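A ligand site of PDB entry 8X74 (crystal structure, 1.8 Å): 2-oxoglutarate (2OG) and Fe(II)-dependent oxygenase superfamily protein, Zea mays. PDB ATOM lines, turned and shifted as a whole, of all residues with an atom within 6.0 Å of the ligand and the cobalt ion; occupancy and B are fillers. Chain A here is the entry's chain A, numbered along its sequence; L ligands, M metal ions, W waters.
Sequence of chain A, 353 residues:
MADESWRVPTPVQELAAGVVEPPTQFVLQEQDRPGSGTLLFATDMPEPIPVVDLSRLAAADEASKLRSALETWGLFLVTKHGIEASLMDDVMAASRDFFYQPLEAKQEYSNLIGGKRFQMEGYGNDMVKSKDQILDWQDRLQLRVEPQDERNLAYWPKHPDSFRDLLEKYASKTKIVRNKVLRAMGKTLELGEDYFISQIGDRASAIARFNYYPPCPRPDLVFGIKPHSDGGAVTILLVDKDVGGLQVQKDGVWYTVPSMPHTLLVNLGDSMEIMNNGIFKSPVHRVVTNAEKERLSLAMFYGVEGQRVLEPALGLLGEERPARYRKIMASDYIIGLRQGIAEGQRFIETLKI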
ATOM      1  N   GLN A 138       2.575  25.040   0.919  1.00  0.00           N
ATOM      2  CA  GLN A 138       2.327  25.477  -0.448  1.00  0.00           C
ATOM      3  C   GLN A 138       0.853  25.314  -0.798  1.00  0.00           C
ATOM      4  O   GLN A 138       0.141  24.494  -0.204  1.00  0.00           O
ATOM      5  CB  GLN A 138       3.175  24.694  -1.471  1.00  0.00           C
ATOM      6  CG  GLN A 138       2.633  23.279  -1.802  1.00  0.00           C
ATOM      7  CD  GLN A 138       3.057  22.796  -3.197  1.00  0.00           C
ATOM      8  OE1 GLN A 138       3.444  21.644  -3.393  1.00  0.00           O
ATOM      9  NE2 GLN A 138       2.991  23.679  -4.168  1.00  0.00           N
ATOM     10  N   ARG A 209       1.239  22.336 -13.332  1.00  0.00           N
ATOM     11  CA  ARG A 209       1.102  22.558 -11.896  1.00  0.00           C
ATOM     12  C   ARG A 209       1.790  23.869 -11.547  1.00  0.00           C
ATOM     13  O   ARG A 209       3.020  23.973 -11.638  1.00  0.00           O
ATOM     14  CB  ARG A 209       1.674  21.398 -11.094  1.00  0.00           C
ATOM     15  CG  ARG A 209       1.652  21.625  -9.574  1.00  0.00           C
ATOM     16  CD  ARG A 209       2.183  20.382  -8.861  1.00  0.00           C
ATOM     17  NE  ARG A 209       2.241  20.571  -7.404  1.00  0.00           N
ATOM     18  CZ  ARG A 209       1.524  19.868  -6.517  1.00  0.00           C
ATOM     19  NH1 ARG A 209       0.665  18.945  -6.910  1.00  0.00           N
ATOM     20  NH2 ARG A 209       1.659  20.121  -5.216  1.00  0.00           N
ATOM     21  N   ASN A 211       2.833  26.072  -8.661  1.00  0.00           N
ATOM     22  CA  ASN A 211       3.102  26.000  -7.223  1.00  0.00           C
ATOM     23  C   ASN A 211       3.269  27.390  -6.657  1.00  0.00           C
ATOM     24  O   ASN A 211       3.977  28.218  -7.228  1.00  0.00           O
ATOM     25  CB  ASN A 211       4.368  25.191  -6.951  1.00  0.00           C
ATOM     26  CG  ASN A 211       4.259  23.767  -7.414  1.00  0.00           C
ATOM     27  OD1 ASN A 211       3.446  23.005  -6.901  1.00  0.00           O
ATOM     28  ND2 ASN A 211       5.096  23.394  -8.371  1.00  0.00           N
ATOM     29  N   TYR A 213       4.507  28.968  -3.040  1.00  0.00           N
ATOM     30  CA  TYR A 213       5.056  28.735  -1.708  1.00  0.00           C
ATOM     31  C   TYR A 213       5.083  30.047  -0.950  1.00  0.00           C
ATOM     32  O   TYR A 213       5.929  30.901  -1.245  1.00  0.00           O
ATOM     33  CB  TYR A 213       6.465  28.148  -1.779  1.00  0.00           C
ATOM     34  CG  TYR A 213       6.603  26.938  -2.685  1.00  0.00           C
ATOM     35  CD1 TYR A 213       6.892  27.107  -4.028  1.00  0.00           C
ATOM     36  CD2 TYR A 213       6.475  25.637  -2.172  1.00  0.00           C
ATOM     37  CE1 TYR A 213       7.016  25.999  -4.871  1.00  0.00           C
ATOM     38  CE2 TYR A 213       6.601  24.521  -3.020  1.00  0.00           C
ATOM     39  CZ  TYR A 213       6.870  24.712  -4.349  1.00  0.00           C
ATOM     40  OH  TYR A 213       6.990  23.621  -5.180  1.00  0.00           O
ATOM     41  N   ILE A 225       7.539  21.683  -0.682  1.00  0.00           N
ATOM     42  CA  ILE A 225       6.947  20.450  -1.184  1.00  0.00           C
ATOM     43  C   ILE A 225       7.840  19.300  -0.703  1.00  0.00           C
ATOM     44  O   ILE A 225       9.066  19.408  -0.730  1.00  0.00           O
ATOM     45  CB  ILE A 225       6.770  20.444  -2.730  1.00  0.00           C
ATOM     46  CG1 ILE A 225       5.833  19.308  -3.125  1.00  0.00           C
ATOM     47  CG2 ILE A 225       8.094  20.367  -3.474  1.00  0.00           C
ATOM     48  CD1 ILE A 225       5.388  19.345  -4.606  1.00  0.00           C
ATOM     49  N   HIS A 228       9.930  13.835  -3.086  1.00  0.00           N
ATOM     50  CA  HIS A 228       9.113  13.026  -3.968  1.00  0.00           C
ATOM     51  C   HIS A 228       9.843  12.884  -5.292  1.00  0.00           C
ATOM     52  O   HIS A 228      10.756  13.663  -5.601  1.00  0.00           O
ATOM     53  CB  HIS A 228       7.733  13.680  -4.196  1.00  0.00           C
ATOM     54  CG  HIS A 228       7.800  14.918  -5.030  1.00  0.00           C
ATOM     55  ND1 HIS A 228       8.213  16.120  -4.523  1.00  0.00           N
ATOM     56  CD2 HIS A 228       7.538  15.124  -6.337  1.00  0.00           C
ATOM     57  CE1 HIS A 228       8.199  17.033  -5.484  1.00  0.00           C
ATOM     58  NE2 HIS A 228       7.801  16.454  -6.598  1.00  0.00           N
ATOM     59  N   SER A 229       9.459  11.884  -6.061  1.00  0.00           N
ATOM     60  CA  SER A 229       9.790  11.855  -7.482  1.00  0.00           C
ATOM     61  C   SER A 229       8.512  12.070  -8.292  1.00  0.00           C
ATOM     62  O   SER A 229       7.408  11.750  -7.831  1.00  0.00           O
ATOM     63  CB  SER A 229      10.489  10.554  -7.895  1.00  0.00           C
ATOM     64  OG  SER A 229       9.722   9.405  -7.541  1.00  0.00           O
ATOM     65  N   ASP A 230       8.658  12.653  -9.475  1.00  0.00           N
ATOM     66  CA  ASP A 230       7.472  12.890 -10.288  1.00  0.00           C
ATOM     67  C   ASP A 230       7.066  11.592 -10.993  1.00  0.00           C
ATOM     68  O   ASP A 230       7.875  10.690 -11.198  1.00  0.00           O
ATOM     69  CB  ASP A 230       7.735  13.953 -11.360  1.00  0.00           C
ATOM     70  CG  ASP A 230       8.133  15.273 -10.796  1.00  0.00           C
ATOM     71  OD1 ASP A 230       7.797  15.566  -9.633  1.00  0.00           O
ATOM     72  OD2 ASP A 230       8.761  16.042 -11.540  1.00  0.00           O
ATOM     73  N   THR A 235       9.638  16.022 -16.661  1.00  0.00           N
ATOM     74  CA  THR A 235       9.030  17.244 -16.140  1.00  0.00           C
ATOM     75  C   THR A 235       9.889  18.401 -16.618  1.00  0.00           C
ATOM     76  O   THR A 235      11.123  18.342 -16.545  1.00  0.00           O
ATOM     77  CB  THR A 235       8.987  17.230 -14.601  1.00  0.00           C
ATOM     78  OG1 THR A 235       8.215  16.115 -14.154  1.00  0.00           O
ATOM     79  CG2 THR A 235       8.432  18.532 -14.017  1.00  0.00           C
ATOM     80  N   LEU A 237      10.438  22.301 -15.764  1.00  0.00           N
ATOM     81  CA  LEU A 237      10.145  23.156 -14.612  1.00  0.00           C
ATOM     82  C   LEU A 237      10.655  24.562 -14.849  1.00  0.00           C
ATOM     83  O   LEU A 237      11.805  24.765 -15.251  1.00  0.00           O
ATOM     84  CB  LEU A 237      10.812  22.598 -13.345  1.00  0.00           C
ATOM     85  CG  LEU A 237      10.659  23.379 -12.041  1.00  0.00           C
ATOM     86  CD1 LEU A 237       9.231  23.235 -11.440  1.00  0.00           C
ATOM     87  CD2 LEU A 237      11.694  22.923 -11.050  1.00  0.00           C
ATOM     88  N   VAL A 239      11.079  28.171 -12.688  1.00  0.00           N
ATOM     89  CA  VAL A 239      11.048  28.788 -11.360  1.00  0.00           C
ATOM     90  C   VAL A 239      11.093  30.294 -11.551  1.00  0.00           C
ATOM     91  O   VAL A 239      12.046  30.823 -12.148  1.00  0.00           O
ATOM     92  CB  VAL A 239      12.196  28.298 -10.461  1.00  0.00           C
ATOM     93  CG1 VAL A 239      12.177  29.024  -9.106  1.00  0.00           C
ATOM     94  CG2 VAL A 239      12.097  26.791 -10.250  1.00  0.00           C
ATOM     95  N   GLY A 245      15.307  27.236  -3.510  1.00  0.00           N
ATOM     96  CA  GLY A 245      14.432  26.364  -2.734  1.00  0.00           C
ATOM     97  C   GLY A 245      14.457  24.929  -3.209  1.00  0.00           C
ATOM     98  O   GLY A 245      14.313  23.998  -2.415  1.00  0.00           O
ATOM     99  N   LEU A 246      14.639  24.747  -4.509  1.00  0.00           N
ATOM    100  CA  LEU A 246      14.612  23.404  -5.080  1.00  0.00           C
ATOM    101  C   LEU A 246      15.892  22.659  -4.718  1.00  0.00           C
ATOM    102  O   LEU A 246      16.986  23.196  -4.834  1.00  0.00           O
ATOM    103  CB  LEU A 246      14.458  23.471  -6.599  1.00  0.00           C
ATOM    104  CG  LEU A 246      14.489  22.113  -7.289  1.00  0.00           C
ATOM    105  CD1 LEU A 246      13.304  21.250  -6.857  1.00  0.00           C
ATOM    106  CD2 LEU A 246      14.507  22.313  -8.801  1.00  0.00           C
ATOM    107  N   ASN A 267      13.701  17.153 -15.517  1.00  0.00           N
ATOM    108  CA  ASN A 267      14.015  16.004 -14.688  1.00  0.00           C
ATOM    109  C   ASN A 267      13.173  14.823 -15.150  1.00  0.00           C
ATOM    110  O   ASN A 267      12.109  14.981 -15.738  1.00  0.00           O
ATOM    111  CB  ASN A 267      13.805  16.281 -13.158  1.00  0.00           C
ATOM    112  CG  ASN A 267      12.345  16.570 -12.764  1.00  0.00           C
ATOM    113  OD1 ASN A 267      11.929  17.738 -12.708  1.00  0.00           O
ATOM    114  ND2 ASN A 267      11.593  15.534 -12.442  1.00  0.00           N
ATOM    115  N   HIS A 285      13.252  14.865  -5.171  1.00  0.00           N
ATOM    116  CA  HIS A 285      13.514  16.294  -5.022  1.00  0.00           C
ATOM    117  C   HIS A 285      12.502  16.883  -4.058  1.00  0.00           C
ATOM    118  O   HIS A 285      11.468  16.289  -3.751  1.00  0.00           O
ATOM    119  CB  HIS A 285      13.497  17.026  -6.401  1.00  0.00           C
ATOM    120  CG  HIS A 285      12.264  16.773  -7.220  1.00  0.00           C
ATOM    121  ND1 HIS A 285      12.051  15.590  -7.903  1.00  0.00           N
ATOM    122  CD2 HIS A 285      11.153  17.533  -7.442  1.00  0.00           C
ATOM    123  CE1 HIS A 285      10.872  15.629  -8.499  1.00  0.00           C
ATOM    124  NE2 HIS A 285      10.314  16.796  -8.239  1.00  0.00           N
ATOM    125  N   ARG A 286      12.817  18.083  -3.562  1.00  0.00           N
ATOM    126  CA  ARG A 286      11.961  18.750  -2.589  1.00  0.00           C
ATOM    127  C   ARG A 286      12.184  20.241  -2.721  1.00  0.00           C
ATOM    128  O   ARG A 286      13.145  20.685  -3.352  1.00  0.00           O
ATOM    129  CB  ARG A 286      12.266  18.283  -1.159  1.00  0.00           C
ATOM    130  CG  ARG A 286      13.638  18.735  -0.690  1.00  0.00           C
ATOM    131  CD  ARG A 286      13.981  18.178   0.704  1.00  0.00           C
ATOM    132  NE  ARG A 286      15.180  18.834   1.216  1.00  0.00           N
ATOM    133  CZ  ARG A 286      15.817  18.465   2.327  1.00  0.00           C
ATOM    134  NH1 ARG A 286      15.371  17.440   3.052  1.00  0.00           N
ATOM    135  NH2 ARG A 286      16.906  19.117   2.721  1.00  0.00           N
ATOM    136  N   VAL A 287      11.301  21.025  -2.085  1.00  0.00           N
ATOM    137  CA  VAL A 287      11.476  22.473  -1.992  1.00  0.00           C
ATOM    138  C   VAL A 287      11.482  22.870  -0.530  1.00  0.00           C
ATOM    139  O   VAL A 287      10.589  22.464   0.230  1.00  0.00           O
ATOM    140  CB  VAL A 287      10.390  23.251  -2.748  1.00  0.00           C
ATOM    141  CG1 VAL A 287      10.561  24.753  -2.538  1.00  0.00           C
ATOM    142  CG2 VAL A 287      10.473  22.941  -4.236  1.00  0.00           C
ATOM    143  N   ARG A 295       7.592  32.048  -3.269  1.00  0.00           N
ATOM    144  CA  ARG A 295       8.276  31.432  -4.406  1.00  0.00           C
ATOM    145  C   ARG A 295       7.227  30.795  -5.307  1.00  0.00           C
ATOM    146  O   ARG A 295       6.263  30.202  -4.819  1.00  0.00           O
ATOM    147  CB  ARG A 295       9.282  30.380  -3.940  1.00  0.00           C
ATOM    148  CG  ARG A 295      10.013  29.617  -5.046  1.00  0.00           C
ATOM    149  CD  ARG A 295      10.951  28.589  -4.404  1.00  0.00           C
ATOM    150  NE  ARG A 295      11.739  27.845  -5.395  1.00  0.00           N
ATOM    151  CZ  ARG A 295      11.289  26.789  -6.071  1.00  0.00           C
ATOM    152  NH1 ARG A 295      10.067  26.326  -5.888  1.00  0.00           N
ATOM    153  NH2 ARG A 295      12.085  26.187  -6.943  1.00  0.00           N
ATOM    154  N   LEU A 296       7.415  30.921  -6.622  1.00  0.00           N
ATOM    155  CA  LEU A 296       6.444  30.395  -7.585  1.00  0.00           C
ATOM    156  C   LEU A 296       7.164  29.577  -8.636  1.00  0.00           C
ATOM    157  O   LEU A 296       8.240  29.957  -9.101  1.00  0.00           O
ATOM    158  CB  LEU A 296       5.660  31.508  -8.300  1.00  0.00           C
ATOM    159  CG  LEU A 296       4.655  32.367  -7.544  1.00  0.00           C
ATOM    160  CD1 LEU A 296       5.367  33.471  -6.783  1.00  0.00           C
ATOM    161  CD2 LEU A 296       3.676  32.968  -8.530  1.00  0.00           C
ATOM    162  N   SER A 297       6.559  28.455  -8.998  1.00  0.00           N
ATOM    163  CA  SER A 297       7.108  27.636 -10.065  1.00  0.00           C
ATOM    164  C   SER A 297       5.975  27.061 -10.887  1.00  0.00           C
ATOM    165  O   SER A 297       4.827  26.962 -10.437  1.00  0.00           O
ATOM    166  CB  SER A 297       7.987  26.519  -9.528  1.00  0.00           C
ATOM    167  OG  SER A 297       7.203  25.544  -8.842  1.00  0.00           O
ATOM    168  N   ALA A 299       5.501  23.562 -13.079  1.00  0.00           N
ATOM    169  CA  ALA A 299       5.951  22.258 -13.552  1.00  0.00           C
ATOM    170  C   ALA A 299       5.019  21.788 -14.655  1.00  0.00           C
ATOM    171  O   ALA A 299       3.796  21.744 -14.469  1.00  0.00           O
ATOM    172  CB  ALA A 299       5.969  21.258 -12.391  1.00  0.00           C
ATOM    173  N   PHE A 301       4.310  18.494 -16.399  1.00  0.00           N
ATOM    174  CA  PHE A 301       4.510  17.055 -16.329  1.00  0.00           C
ATOM    175  C   PHE A 301       4.094  16.431 -17.651  1.00  0.00           C
ATOM    176  O   PHE A 301       2.948  16.594 -18.060  1.00  0.00           O
ATOM    177  CB  PHE A 301       3.692  16.430 -15.196  1.00  0.00           C
ATOM    178  CG  PHE A 301       3.947  17.037 -13.848  1.00  0.00           C
ATOM    179  CD1 PHE A 301       5.183  16.910 -13.231  1.00  0.00           C
ATOM    180  CD2 PHE A 301       2.942  17.717 -13.193  1.00  0.00           C
ATOM    181  CE1 PHE A 301       5.401  17.471 -11.972  1.00  0.00           C
ATOM    182  CE2 PHE A 301       3.166  18.283 -11.938  1.00  0.00           C
ATOM    183  CZ  PHE A 301       4.388  18.155 -11.323  1.00  0.00           C
HETATM  184  C1  LIG L   1       6.487  19.545  -8.494  1.00  0.00           C
HETATM  185  O1  LIG L   1       5.557  20.372  -8.720  1.00  0.00           O
HETATM  186  O2  LIG L   1       6.353  18.293  -8.661  1.00  0.00           O
HETATM  187  C2  LIG L   1       7.798  20.090  -7.982  1.00  0.00           C
HETATM  188  O3  LIG L   1       8.623  19.323  -7.556  1.00  0.00           O
HETATM  189  C3  LIG L   1       8.035  21.600  -8.030  1.00  0.00           C
HETATM  190  C4  LIG L   1       9.486  21.904  -7.677  1.00  0.00           C
HETATM  191  C5  LIG L   1       9.695  23.405  -7.560  1.00  0.00           C
HETATM  192  O4  LIG L   1       8.753  24.164  -7.157  1.00  0.00           O
HETATM  193  O5  LIG L   1      10.823  23.870  -7.829  1.00  0.00           O
HETATM  194 CO    CO M   1       8.250  17.332  -8.483  1.00  0.00          CO
HETATM  195  O   HOH W   1       8.806  18.366 -10.290  1.00  0.00           O
HETATM  196  O   HOH W   2       4.757  15.190  -8.737  1.00  0.00           O
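O4 of the ligand lies within hydrogen-bond range of OG of Ser 297 (2.7 Å).
O4 of the ligand is in hydrogen-bond range of OH of Tyr 213 (2.7 Å).
NH2 of Arg 295 is in salt-bridge range of O5 of the ligand, at 2.8 Å.
An oxygen (O1) of the ligand is in hydrogen-bond range of the side-chain amide nitrogen (ND2) of Asn 211 (3.1 Å).
The guanidinium group (NE) of Arg 209 lies within salt-bridge range of an oxygen (O1) of the ligand, 3.6 Å away.
The side-chain amide nitrogen (ND2) of Asn 267 sits at hydrogen-bond distance from the side-chain carboxylate (OD2) of Asp 230 (3.0 Å).
The side-chain carboxylate (OD2) of Asp 230 lies within hydrogen-bond range of the side-chain hydroxyl (OG1) of Thr 235, at 2.7 Å.
The backbone carbonyl oxygen of Ser 297 sits at hydrogen-bond distance from the backbone NH of Asn 211 (2.8 Å).
The backbone carbonyl oxygen (O) of Arg 295 sits at hydrogen-bond distance from the backbone NH (N) of Tyr 213 (2.8 Å).
The side-chain amide oxygen of Asn 211 is in hydrogen-bond range of the guanidinium group of Arg 209 (2.8 Å).
The backbone NH of Arg 209 is in hydrogen-bond range of the backbone carbonyl oxygen of Ala 299 (2.9 Å).
NH2 of Arg 209 lies within hydrogen-bond range of OE1 of Gln 138.
N of Val 287 sits at hydrogen-bond distance from O of Ile 225, 3.1 Å away.
Residues that only touch the ligand: Phe 301, Val 287, Leu 237, Leu 246 and Ala 299.
Hydrophobic or aromatic side chains that line the ligand: Tyr 213, His 228, Leu 237, Leu 246, His 285, Val 287, Ala 299 and Phe 301.
Within 4 Å of the ligand: Arg 209, Asn 211, Tyr 213, His 228, Asp 230, Leu 237, Leu 246, His 285, Val 287, Arg 295, Ser 297, Ala 299 and Phe 301.
The nearest printed residue that does not touch the ligand is Val 239 (4.002 Å).
Three residues have an atom within 4 Å of the cobalt ion: His 228, Asp 230 and His 285.
The nearest printed residue that does not touch the cobalt ion is Phe 301 (4.5 Å).
The cobalt ion is bound by a ring nitrogen (NE2) of His 228 (2.1 Å).
An oxygen (O2) of the ligand is bound to the cobalt ion (2.1 Å).
The cobalt ion is bound by NE2 of His 285.
Water W1 is bound to the cobalt ion (2.2 Å).
The cobalt ion is bound by the side-chain carboxylate (OD1) of Asp 230 (2.2 Å).
O3 of the ligand binds the cobalt ion (2.2 Å).
The cobalt ion has six donor atoms within binding distance.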
